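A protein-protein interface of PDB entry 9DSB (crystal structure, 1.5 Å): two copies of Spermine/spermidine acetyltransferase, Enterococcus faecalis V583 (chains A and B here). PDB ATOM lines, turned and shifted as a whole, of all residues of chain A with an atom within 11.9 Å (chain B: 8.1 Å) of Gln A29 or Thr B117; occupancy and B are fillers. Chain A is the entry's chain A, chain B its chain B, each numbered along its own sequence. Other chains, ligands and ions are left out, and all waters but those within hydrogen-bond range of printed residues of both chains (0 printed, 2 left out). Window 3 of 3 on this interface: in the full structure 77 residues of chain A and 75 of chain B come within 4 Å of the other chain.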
ATOM      1  N   VAL A  24      34.057   2.346  22.182  1.00  0.00           N
ATOM      2  CA  VAL A  24      33.041   2.989  23.007  1.00  0.00           C
ATOM      3  C   VAL A  24      32.996   2.357  24.404  1.00  0.00           C
ATOM      4  O   VAL A  24      31.925   2.265  25.000  1.00  0.00           O
ATOM      5  CB  VAL A  24      31.672   2.888  22.298  1.00  0.00           C
ATOM      6  CG1 VAL A  24      31.513   3.901  21.169  1.00  0.00           C
ATOM      7  CG2 VAL A  24      31.391   1.478  21.785  1.00  0.00           C
ATOM      8  N   PHE A  25      34.168   2.001  24.954  1.00  0.00           N
ATOM      9  CA  PHE A  25      34.280   1.131  26.121  1.00  0.00           C
ATOM     10  C   PHE A  25      34.363   1.925  27.429  1.00  0.00           C
ATOM     11  O   PHE A  25      35.039   1.496  28.363  1.00  0.00           O
ATOM     12  CB  PHE A  25      35.537   0.248  26.085  1.00  0.00           C
ATOM     13  CG  PHE A  25      36.075  -0.131  24.711  1.00  0.00           C
ATOM     14  CD1 PHE A  25      35.222  -0.522  23.686  1.00  0.00           C
ATOM     15  CD2 PHE A  25      37.442  -0.077  24.446  1.00  0.00           C
ATOM     16  CE1 PHE A  25      35.721  -0.852  22.434  1.00  0.00           C
ATOM     17  CE2 PHE A  25      37.935  -0.398  23.190  1.00  0.00           C
ATOM     18  CZ  PHE A  25      37.076  -0.789  22.189  1.00  0.00           C
ATOM     19  N   ALA A  26      33.690   3.076  27.505  1.00  0.00           N
ATOM     20  CA  ALA A  26      33.569   3.800  28.762  1.00  0.00           C
ATOM     21  C   ALA A  26      32.247   4.561  28.820  1.00  0.00           C
ATOM     22  O   ALA A  26      31.843   5.019  29.886  1.00  0.00           O
ATOM     23  CB  ALA A  26      34.741   4.738  28.931  1.00  0.00           C
ATOM     24  N   GLU A  27      31.582   4.672  27.667  1.00  0.00           N
ATOM     25  CA  GLU A  27      30.396   5.494  27.519  1.00  0.00           C
ATOM     26  C   GLU A  27      29.225   4.746  28.151  1.00  0.00           C
ATOM     27  O   GLU A  27      28.411   4.145  27.452  1.00  0.00           O
ATOM     28  CB  GLU A  27      30.185   5.794  26.034  1.00  0.00           C
ATOM     29  CG  GLU A  27      31.480   6.031  25.260  1.00  0.00           C
ATOM     30  CD  GLU A  27      31.318   6.630  23.875  1.00  0.00           C
ATOM     31  OE1 GLU A  27      30.169   6.827  23.427  1.00  0.00           O
ATOM     32  OE2 GLU A  27      32.356   6.895  23.236  1.00  0.00           O
ATOM     33  N   GLN A  28      29.169   4.774  29.486  1.00  0.00           N
ATOM     34  CA  GLN A  28      28.181   4.020  30.241  1.00  0.00           C
ATOM     35  C   GLN A  28      26.789   4.553  29.914  1.00  0.00           C
ATOM     36  O   GLN A  28      25.860   3.777  29.711  1.00  0.00           O
ATOM     37  CB  GLN A  28      28.492   4.120  31.734  1.00  0.00           C
ATOM     38  CG  GLN A  28      29.874   3.595  32.119  1.00  0.00           C
ATOM     39  CD  GLN A  28      30.596   4.493  33.100  1.00  0.00           C
ATOM     40  OE1 GLN A  28      31.703   4.978  32.837  1.00  0.00           O
ATOM     41  NE2 GLN A  28      29.969   4.734  34.244  1.00  0.00           N
ATOM     42  N   GLN A  29      26.664   5.886  29.850  1.00  0.00           N
ATOM     43  CA  GLN A  29      25.403   6.526  29.509  1.00  0.00           C
ATOM     44  C   GLN A  29      25.031   6.222  28.060  1.00  0.00           C
ATOM     45  O   GLN A  29      23.850   6.080  27.747  1.00  0.00           O
ATOM     46  CB  GLN A  29      25.445   8.033  29.775  1.00  0.00           C
ATOM     47  CG  GLN A  29      25.048   8.419  31.197  1.00  0.00           C
ATOM     48  CD  GLN A  29      23.573   8.223  31.483  1.00  0.00           C
ATOM     49  OE1 GLN A  29      22.761   7.996  30.578  1.00  0.00           O
ATOM     50  NE2 GLN A  29      23.208   8.319  32.753  1.00  0.00           N
ATOM     51  N   ALA A  30      26.035   6.119  27.182  1.00  0.00           N
ATOM     52  CA  ALA A  30      25.787   5.833  25.778  1.00  0.00           C
ATOM     53  C   ALA A  30      25.177   4.443  25.621  1.00  0.00           C
ATOM     54  O   ALA A  30      24.254   4.266  24.832  1.00  0.00           O
ATOM     55  CB  ALA A  30      27.056   5.963  24.969  1.00  0.00           C
ATOM     56  N   PHE A  31      25.696   3.456  26.361  1.00  0.00           N
ATOM     57  CA  PHE A  31      25.233   2.088  26.184  1.00  0.00           C
ATOM     58  C   PHE A  31      23.831   1.938  26.771  1.00  0.00           C
ATOM     59  O   PHE A  31      23.072   1.085  26.319  1.00  0.00           O
ATOM     60  CB  PHE A  31      26.137   0.997  26.766  1.00  0.00           C
ATOM     61  CG  PHE A  31      25.931  -0.336  26.054  1.00  0.00           C
ATOM     62  CD1 PHE A  31      25.010  -1.269  26.521  1.00  0.00           C
ATOM     63  CD2 PHE A  31      26.626  -0.629  24.885  1.00  0.00           C
ATOM     64  CE1 PHE A  31      24.818  -2.470  25.849  1.00  0.00           C
ATOM     65  CE2 PHE A  31      26.426  -1.829  24.220  1.00  0.00           C
ATOM     66  CZ  PHE A  31      25.522  -2.743  24.700  1.00  0.00           C
ATOM     67  N   ILE A  32      23.488   2.772  27.765  1.00  0.00           N
ATOM     68  CA  ILE A  32      22.117   2.845  28.244  1.00  0.00           C
ATOM     69  C   ILE A  32      21.211   3.209  27.071  1.00  0.00           C
ATOM     70  O   ILE A  32      20.166   2.596  26.880  1.00  0.00           O
ATOM     71  CB  ILE A  32      21.962   3.830  29.420  1.00  0.00           C
ATOM     72  CG1 ILE A  32      22.673   3.325  30.678  1.00  0.00           C
ATOM     73  CG2 ILE A  32      20.486   4.121  29.694  1.00  0.00           C
ATOM     74  CD1 ILE A  32      22.717   4.332  31.815  1.00  0.00           C
ATOM     75  N   GLU A  33      21.625   4.211  26.285  1.00  0.00           N
ATOM     76  CA  GLU A  33      20.847   4.648  25.137  1.00  0.00           C
ATOM     77  C   GLU A  33      20.827   3.550  24.077  1.00  0.00           C
ATOM     78  O   GLU A  33      19.808   3.346  23.422  1.00  0.00           O
ATOM     79  CB  GLU A  33      21.384   5.963  24.570  1.00  0.00           C
ATOM     80  CG  GLU A  33      21.354   7.117  25.569  1.00  0.00           C
ATOM     81  CD  GLU A  33      19.969   7.502  26.057  1.00  0.00           C
ATOM     82  OE1 GLU A  33      18.971   7.069  25.440  1.00  0.00           O
ATOM     83  OE2 GLU A  33      19.886   8.210  27.087  1.00  0.00           O
ATOM     84  N   SER A  34      21.954   2.851  23.901  1.00  0.00           N
ATOM     85  CA  SER A  34      22.022   1.767  22.934  1.00  0.00           C
ATOM     86  C   SER A  34      21.000   0.687  23.269  1.00  0.00           C
ATOM     87  O   SER A  34      20.309   0.186  22.385  1.00  0.00           O
ATOM     88  CB  SER A  34      23.407   1.173  22.844  1.00  0.00           C
ATOM     89  OG  SER A  34      23.727   0.841  21.495  1.00  0.00           O
ATOM     90  N   MET A  35      20.913   0.335  24.554  1.00  0.00           N
ATOM     91  CA  MET A  35      20.017  -0.724  24.987  1.00  0.00           C
ATOM     92  C   MET A  35      18.567  -0.264  24.849  1.00  0.00           C
ATOM     93  O   MET A  35      17.715  -1.033  24.414  1.00  0.00           O
ATOM     94  CB  MET A  35      20.315  -1.152  26.427  1.00  0.00           C
ATOM     95  CG  MET A  35      19.524  -2.370  26.885  1.00  0.00           C
ATOM     96  SD  MET A  35      19.707  -3.847  25.864  1.00  0.00           S
ATOM     97  CE  MET A  35      21.485  -4.096  25.952  1.00  0.00           C
ATOM     98  N   ALA A  36      18.288   0.991  25.227  1.00  0.00           N
ATOM     99  CA  ALA A  36      16.942   1.529  25.116  1.00  0.00           C
ATOM    100  C   ALA A  36      16.459   1.454  23.670  1.00  0.00           C
ATOM    101  O   ALA A  36      15.307   1.130  23.407  1.00  0.00           O
ATOM    102  CB  ALA A  36      16.896   2.940  25.656  1.00  0.00           C
ATOM    103  N   GLU A  37      17.353   1.742  22.724  1.00  0.00           N
ATOM    104  CA  GLU A  37      17.003   1.654  21.317  1.00  0.00           C
ATOM    105  C   GLU A  37      16.864   0.185  20.919  1.00  0.00           C
ATOM    106  O   GLU A  37      15.931  -0.159  20.199  1.00  0.00           O
ATOM    107  CB  GLU A  37      17.998   2.425  20.451  1.00  0.00           C
ATOM    108  CG  GLU A  37      17.651   2.405  18.965  1.00  0.00           C
ATOM    109  CD  GLU A  37      16.323   3.026  18.569  1.00  0.00           C
ATOM    110  OE1 GLU A  37      15.762   3.781  19.382  1.00  0.00           O
ATOM    111  OE2 GLU A  37      15.841   2.753  17.444  1.00  0.00           O
ATOM    112  N   ASN A  38      17.787  -0.676  21.379  1.00  0.00           N
ATOM    113  CA  ASN A  38      17.679  -2.110  21.140  1.00  0.00           C
ATOM    114  C   ASN A  38      16.274  -2.586  21.504  1.00  0.00           C
ATOM    115  O   ASN A  38      15.632  -3.292  20.727  1.00  0.00           O
ATOM    116  CB  ASN A  38      18.682  -2.946  21.936  1.00  0.00           C
ATOM    117  CG  ASN A  38      20.108  -2.800  21.463  1.00  0.00           C
ATOM    118  OD1 ASN A  38      20.361  -2.269  20.377  1.00  0.00           O
ATOM    119  ND2 ASN A  38      21.047  -3.292  22.260  1.00  0.00           N
ATOM    120  N   GLU B  20      18.182  -1.883  30.604  1.00  0.00           N
ATOM    121  CA  GLU B  20      18.858  -0.760  29.971  1.00  0.00           C
ATOM    122  C   GLU B  20      20.157  -0.419  30.701  1.00  0.00           C
ATOM    123  O   GLU B  20      21.056   0.164  30.100  1.00  0.00           O
ATOM    124  CB  GLU B  20      17.921   0.442  29.860  1.00  0.00           C
ATOM    125  CG  GLU B  20      16.815   0.221  28.832  1.00  0.00           C
ATOM    126  CD  GLU B  20      15.691   1.235  28.874  1.00  0.00           C
ATOM    127  OE1 GLU B  20      15.677   2.112  29.773  1.00  0.00           O
ATOM    128  OE2 GLU B  20      14.815   1.142  27.987  1.00  0.00           O
ATOM    129  N   ASN B  21      20.262  -0.807  31.979  1.00  0.00           N
ATOM    130  CA  ASN B  21      21.404  -0.468  32.815  1.00  0.00           C
ATOM    131  C   ASN B  21      22.369  -1.650  32.963  1.00  0.00           C
ATOM    132  O   ASN B  21      23.313  -1.568  33.743  1.00  0.00           O
ATOM    133  CB  ASN B  21      20.937   0.068  34.165  1.00  0.00           C
ATOM    134  CG  ASN B  21      20.562   1.529  34.081  1.00  0.00           C
ATOM    135  OD1 ASN B  21      21.448   2.389  34.035  1.00  0.00           O
ATOM    136  ND2 ASN B  21      19.273   1.829  34.039  1.00  0.00           N
ATOM    137  N   PHE B  25      29.395  -2.175  29.540  1.00  0.00           N
ATOM    138  CA  PHE B  25      30.032  -1.004  28.952  1.00  0.00           C
ATOM    139  C   PHE B  25      31.550  -1.183  28.863  1.00  0.00           C
ATOM    140  O   PHE B  25      32.235  -0.320  28.310  1.00  0.00           O
ATOM    141  CB  PHE B  25      29.726   0.262  29.760  1.00  0.00           C
ATOM    142  CG  PHE B  25      30.250   0.244  31.189  1.00  0.00           C
ATOM    143  CD1 PHE B  25      31.538   0.675  31.486  1.00  0.00           C
ATOM    144  CD2 PHE B  25      29.451  -0.208  32.233  1.00  0.00           C
ATOM    145  CE1 PHE B  25      32.012   0.651  32.789  1.00  0.00           C
ATOM    146  CE2 PHE B  25      29.929  -0.230  33.534  1.00  0.00           C
ATOM    147  CZ  PHE B  25      31.206   0.200  33.808  1.00  0.00           C
ATOM    148  N   PHE B  78      23.316   7.449  18.148  1.00  0.00           N
ATOM    149  CA  PHE B  78      24.328   8.468  17.940  1.00  0.00           C
ATOM    150  C   PHE B  78      25.474   8.221  18.915  1.00  0.00           C
ATOM    151  O   PHE B  78      25.279   8.265  20.127  1.00  0.00           O
ATOM    152  CB  PHE B  78      23.722   9.864  18.110  1.00  0.00           C
ATOM    153  CG  PHE B  78      24.703  10.969  17.754  1.00  0.00           C
ATOM    154  CD1 PHE B  78      24.870  11.371  16.434  1.00  0.00           C
ATOM    155  CD2 PHE B  78      25.470  11.589  18.737  1.00  0.00           C
ATOM    156  CE1 PHE B  78      25.776  12.365  16.105  1.00  0.00           C
ATOM    157  CE2 PHE B  78      26.372  12.588  18.403  1.00  0.00           C
ATOM    158  CZ  PHE B  78      26.524  12.974  17.090  1.00  0.00           C
ATOM    159  N   LEU B  79      26.658   7.943  18.361  1.00  0.00           N
ATOM    160  CA  LEU B  79      27.826   7.562  19.139  1.00  0.00           C
ATOM    161  C   LEU B  79      29.049   8.277  18.582  1.00  0.00           C
ATOM    162  O   LEU B  79      29.237   8.325  17.368  1.00  0.00           O
ATOM    163  CB  LEU B  79      28.070   6.054  19.092  1.00  0.00           C
ATOM    164  CG  LEU B  79      27.014   5.157  19.738  1.00  0.00           C
ATOM    165  CD1 LEU B  79      27.337   3.723  19.364  1.00  0.00           C
ATOM    166  CD2 LEU B  79      26.953   5.318  21.250  1.00  0.00           C
ATOM    167  N   VAL B 114      15.573  10.138  25.407  1.00  0.00           N
ATOM    168  CA  VAL B 114      16.749  10.074  26.260  1.00  0.00           C
ATOM    169  C   VAL B 114      16.376   9.478  27.615  1.00  0.00           C
ATOM    170  O   VAL B 114      15.251   9.633  28.091  1.00  0.00           O
ATOM    171  CB  VAL B 114      17.381  11.469  26.437  1.00  0.00           C
ATOM    172  CG1 VAL B 114      18.176  11.882  25.211  1.00  0.00           C
ATOM    173  CG2 VAL B 114      16.345  12.528  26.790  1.00  0.00           C
ATOM    174  N   TYR B 115      17.362   8.814  28.230  1.00  0.00           N
ATOM    175  CA  TYR B 115      17.251   8.336  29.596  1.00  0.00           C
ATOM    176  C   TYR B 115      17.459   9.531  30.524  1.00  0.00           C
ATOM    177  O   TYR B 115      18.238  10.432  30.215  1.00  0.00           O
ATOM    178  CB  TYR B 115      18.253   7.204  29.840  1.00  0.00           C
ATOM    179  CG  TYR B 115      17.916   6.337  31.046  1.00  0.00           C
ATOM    180  CD1 TYR B 115      17.085   5.228  30.926  1.00  0.00           C
ATOM    181  CD2 TYR B 115      18.414   6.638  32.307  1.00  0.00           C
ATOM    182  CE1 TYR B 115      16.775   4.436  32.020  1.00  0.00           C
ATOM    183  CE2 TYR B 115      18.107   5.858  33.412  1.00  0.00           C
ATOM    184  CZ  TYR B 115      17.279   4.757  33.269  1.00  0.00           C
ATOM    185  OH  TYR B 115      16.976   3.988  34.356  1.00  0.00           O
ATOM    186  N   ASP B 116      16.763   9.518  31.665  1.00  0.00           N
ATOM    187  CA  ASP B 116      16.662  10.688  32.525  1.00  0.00           C
ATOM    188  C   ASP B 116      18.027  11.076  33.087  1.00  0.00           C
ATOM    189  O   ASP B 116      18.368  12.258  33.108  1.00  0.00           O
ATOM    190  CB  ASP B 116      15.629  10.474  33.617  1.00  0.00           C
ATOM    191  CG  ASP B 116      14.187  10.453  33.132  1.00  0.00           C
ATOM    192  OD1 ASP B 116      13.980  10.642  31.916  1.00  0.00           O
ATOM    193  OD2 ASP B 116      13.290  10.254  33.978  1.00  0.00           O
ATOM    194  N   THR B 117      18.804  10.078  33.528  1.00  0.00           N
ATOM    195  CA  THR B 117      20.083  10.319  34.181  1.00  0.00           C
ATOM    196  C   THR B 117      21.155  10.708  33.161  1.00  0.00           C
ATOM    197  O   THR B 117      22.292  10.974  33.548  1.00  0.00           O
ATOM    198  CB  THR B 117      20.505   9.088  34.988  1.00  0.00           C
ATOM    199  OG1 THR B 117      20.717   8.020  34.069  1.00  0.00           O
ATOM    200  CG2 THR B 117      19.474   8.684  36.028  1.00  0.00           C
ATOM    201  N   ASN B 118      20.801  10.731  31.868  1.00  0.00           N
ATOM    202  CA  ASN B 118      21.723  11.143  30.820  1.00  0.00           C
ATOM    203  C   ASN B 118      21.790  12.668  30.791  1.00  0.00           C
ATOM    204  O   ASN B 118      21.006  13.315  30.099  1.00  0.00           O
ATOM    205  CB  ASN B 118      21.321  10.548  29.473  1.00  0.00           C
ATOM    206  CG  ASN B 118      22.469  10.484  28.493  1.00  0.00           C
ATOM    207  OD1 ASN B 118      23.538  11.059  28.733  1.00  0.00           O
ATOM    208  ND2 ASN B 118      22.267   9.802  27.376  1.00  0.00           N
ATOM    209  N   SER B 119      22.746  13.228  31.543  1.00  0.00           N
ATOM    210  CA  SER B 119      22.845  14.666  31.742  1.00  0.00           C
ATOM    211  C   SER B 119      23.532  15.334  30.552  1.00  0.00           C
ATOM    212  O   SER B 119      23.104  16.400  30.114  1.00  0.00           O
ATOM    213  CB  SER B 119      23.561  14.976  33.034  1.00  0.00           C
ATOM    214  OG  SER B 119      22.919  14.342  34.132  1.00  0.00           O
ATOM    215  N   SER B 120      24.603  14.709  30.046  1.00  0.00           N
ATOM    216  CA  SER B 120      25.348  15.241  28.915  1.00  0.00           C
ATOM    217  C   SER B 120      24.456  15.317  27.679  1.00  0.00           C
ATOM    218  O   SER B 120      24.500  16.306  26.950  1.00  0.00           O
ATOM    219  CB  SER B 120      26.590  14.427  28.638  1.00  0.00           C
ATOM    220  OG  SER B 120      27.495  14.483  29.732  1.00  0.00           O
ATOM    221  N   ALA B 121      23.644  14.272  27.466  1.00  0.00           N
ATOM    222  CA  ALA B 121      22.820  14.163  26.272  1.00  0.00           C
ATOM    223  C   ALA B 121      21.714  15.214  26.285  1.00  0.00           C
ATOM    224  O   ALA B 121      21.498  15.888  25.282  1.00  0.00           O
ATOM    225  CB  ALA B 121      22.248  12.769  26.153  1.00  0.00           C
ATOM    226  N   ILE B 122      21.016  15.341  27.420  1.00  0.00           N
ATOM    227  CA  ILE B 122      19.942  16.314  27.550  1.00  0.00           C
ATOM    228  C   ILE B 122      20.507  17.717  27.326  1.00  0.00           C
ATOM    229  O   ILE B 122      19.922  18.494  26.577  1.00  0.00           O
ATOM    230  CB  ILE B 122      19.214  16.166  28.902  1.00  0.00           C
ATOM    231  CG1 ILE B 122      18.468  14.830  28.977  1.00  0.00           C
ATOM    232  CG2 ILE B 122      18.271  17.345  29.156  1.00  0.00           C
ATOM    233  CD1 ILE B 122      17.942  14.470  30.357  1.00  0.00           C
ATOM    234  N   ARG B 123      21.650  18.018  27.957  1.00  0.00           N
ATOM    235  CA  ARG B 123      22.338  19.285  27.761  1.00  0.00           C
ATOM    236  C   ARG B 123      22.650  19.483  26.279  1.00  0.00           C
ATOM    237  O   ARG B 123      22.228  20.475  25.689  1.00  0.00           O
ATOM    238  CB  ARG B 123      23.620  19.366  28.599  1.00  0.00           C
ATOM    239  CG  ARG B 123      23.387  19.819  30.034  1.00  0.00           C
ATOM    240  CD  ARG B 123      24.642  19.771  30.899  1.00  0.00           C
ATOM    241  NE  ARG B 123      25.153  18.406  31.075  1.00  0.00           N
ATOM    242  CZ  ARG B 123      26.098  18.032  31.935  1.00  0.00           C
ATOM    243  NH1 ARG B 123      26.619  18.900  32.785  1.00  0.00           N
ATOM    244  NH2 ARG B 123      26.509  16.776  31.959  1.00  0.00           N
ATOM    245  N   GLU B 141      11.457   6.143  27.689  1.00  0.00           N
ATOM    246  CA  GLU B 141      12.333   7.306  27.630  1.00  0.00           C
ATOM    247  C   GLU B 141      11.506   8.553  27.312  1.00  0.00           C
ATOM    248  O   GLU B 141      10.498   8.479  26.611  1.00  0.00           O
ATOM    249  CB  GLU B 141      13.463   7.149  26.613  1.00  0.00           C
ATOM    250  CG  GLU B 141      14.501   6.106  27.017  1.00  0.00           C
ATOM    251  CD  GLU B 141      15.746   6.147  26.155  1.00  0.00           C
ATOM    252  OE1 GLU B 141      15.586   6.073  24.917  1.00  0.00           O
ATOM    253  OE2 GLU B 141      16.865   6.258  26.702  1.00  0.00           O
ATOM    254  N   ARG B 142      11.962   9.699  27.829  1.00  0.00           N
ATOM    255  CA  ARG B 142      11.319  10.981  27.583  1.00  0.00           C
ATOM    256  C   ARG B 142      11.715  11.493  26.203  1.00  0.00           C
ATOM    257  O   ARG B 142      12.896  11.530  25.855  1.00  0.00           O
ATOM    258  CB  ARG B 142      11.687  11.998  28.666  1.00  0.00           C
ATOM    259  CG  ARG B 142      10.901  11.760  29.947  1.00  0.00           C
ATOM    260  CD  ARG B 142      11.512  12.469  31.142  1.00  0.00           C
ATOM    261  NE  ARG B 142      11.610  13.920  30.966  1.00  0.00           N
ATOM    262  CZ  ARG B 142      12.416  14.729  31.651  1.00  0.00           C
ATOM    263  NH1 ARG B 142      13.313  14.242  32.494  1.00  0.00           N
ATOM    264  NH2 ARG B 142      12.338  16.035  31.474  1.00  0.00           N
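Phe B25 touches its own counterpart, Phe A25.
Of the 16 pairs that touch across the chains among the printed residues, 1 has its exchanged pair printed and touching as well.
OG1 of Thr B117 lies within hydrogen-bond range of NE2 of Gln A29 (2.8 Å).
The side-chain carboxylate of Glu A33 sits at hydrogen-bond distance from the backbone NH of Tyr B115, at 2.8 Å.
OE2 of Glu A33 lies within hydrogen-bond range of ND2 of Asn B118, 2.9 Å away.
The side-chain carboxylate (OE1) of Glu A33 lies close to the side-chain carboxylate (OE2) of Glu B141 (2.6 Å).
The backbone carbonyl oxygen (O) of Phe A25 sits close to the backbone carbonyl oxygen (O) of Phe B25 (3.3 Å).
N of Ala A26 touches O of Phe B25, at 3.8 Å.
Gln A28 touches Phe B25.
Asn B118 touches Gln A29.
Ala A30 touches Leu B79 (CB to CD2, 3.8 Å).
Asn B21 touches Ile A32 (OD1 to CD1, 3.2 Å).
CG2 of Ile A32 touches CG of Tyr B115 (3.7 Å).
Glu A33 touches Val B114.
Met A35 touches Glu B20.
CA of Ala A36 touches OE2 of Glu B20 (3.6 Å).
Ala A36 touches Glu B141.
Of the 17 printed residues of chain B, 9 touch a printed residue of chain A.
Hydrophobic or aromatic side chains of chain B that line the printed part of chain A: Phe B25, Leu B79 and Tyr B115.
Printed residues of chain A that touch a printed residue of chain B: Phe A25, Ala A26, Gln A28, Gln A29, Ala A30, Ile A32, Glu A33, Met A35 and Ala A36.
Among the printed residues, 16 pairs touch across the chains.
The backbone carbonyl oxygen (O) of Ala A26 sits close to the side-chain amide oxygen (OE1) of Gln A28.
The side-chain amide nitrogen (ND2) of Asn B21 sits at hydrogen-bond distance from the side-chain hydroxyl (OH) of Tyr B115 (3.2 Å).
N of Val B114 is in hydrogen-bond range of O of Arg B142, at 3.1 Å.
The side-chain carboxylate of Glu B141 lies within hydrogen-bond range of the backbone NH of Tyr B115 (3.0 Å).
OG of Ser B119 is in hydrogen-bond range of O of Thr B117 (3.5 Å).
OD1 of Asn B118 lies close to N of Ala B121.
Of chain B, only Thr B117 and Asn B118 come within 4 Å of Gln A29.
Printed residues of chain B within 4 Å of Ala A30: Leu B79 (3.8 Å).
Asn A38 touches none of the printed residues of chain B.
Of the printed residues of chain A, Glu B20 touches Ile A32, Met A35 and Ala A36.
Of the printed residues of chain A, Phe B25 touches Phe A25 (3.2 Å), Ala A26 (3.8 Å) and Gln A28 (3.4 Å).
Printed residues of chain A within 4 Å of Leu B79: Ala A30.
Tyr B115 touches just these residues of chain A: Ile A32 (3.7 Å) and Glu A33 (2.8 Å).
Asp B116 touches none of the printed residues of chain A.
Of the printed residues of chain A, Thr B117 touches Gln A29.
Asn B118 touches two residues of chain A.
No residue of chain A comes within 4 Å of Ser B119.
The nearest printed residue of chain B that does not touch Ala A36 is Tyr B115 (5.7 Å).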
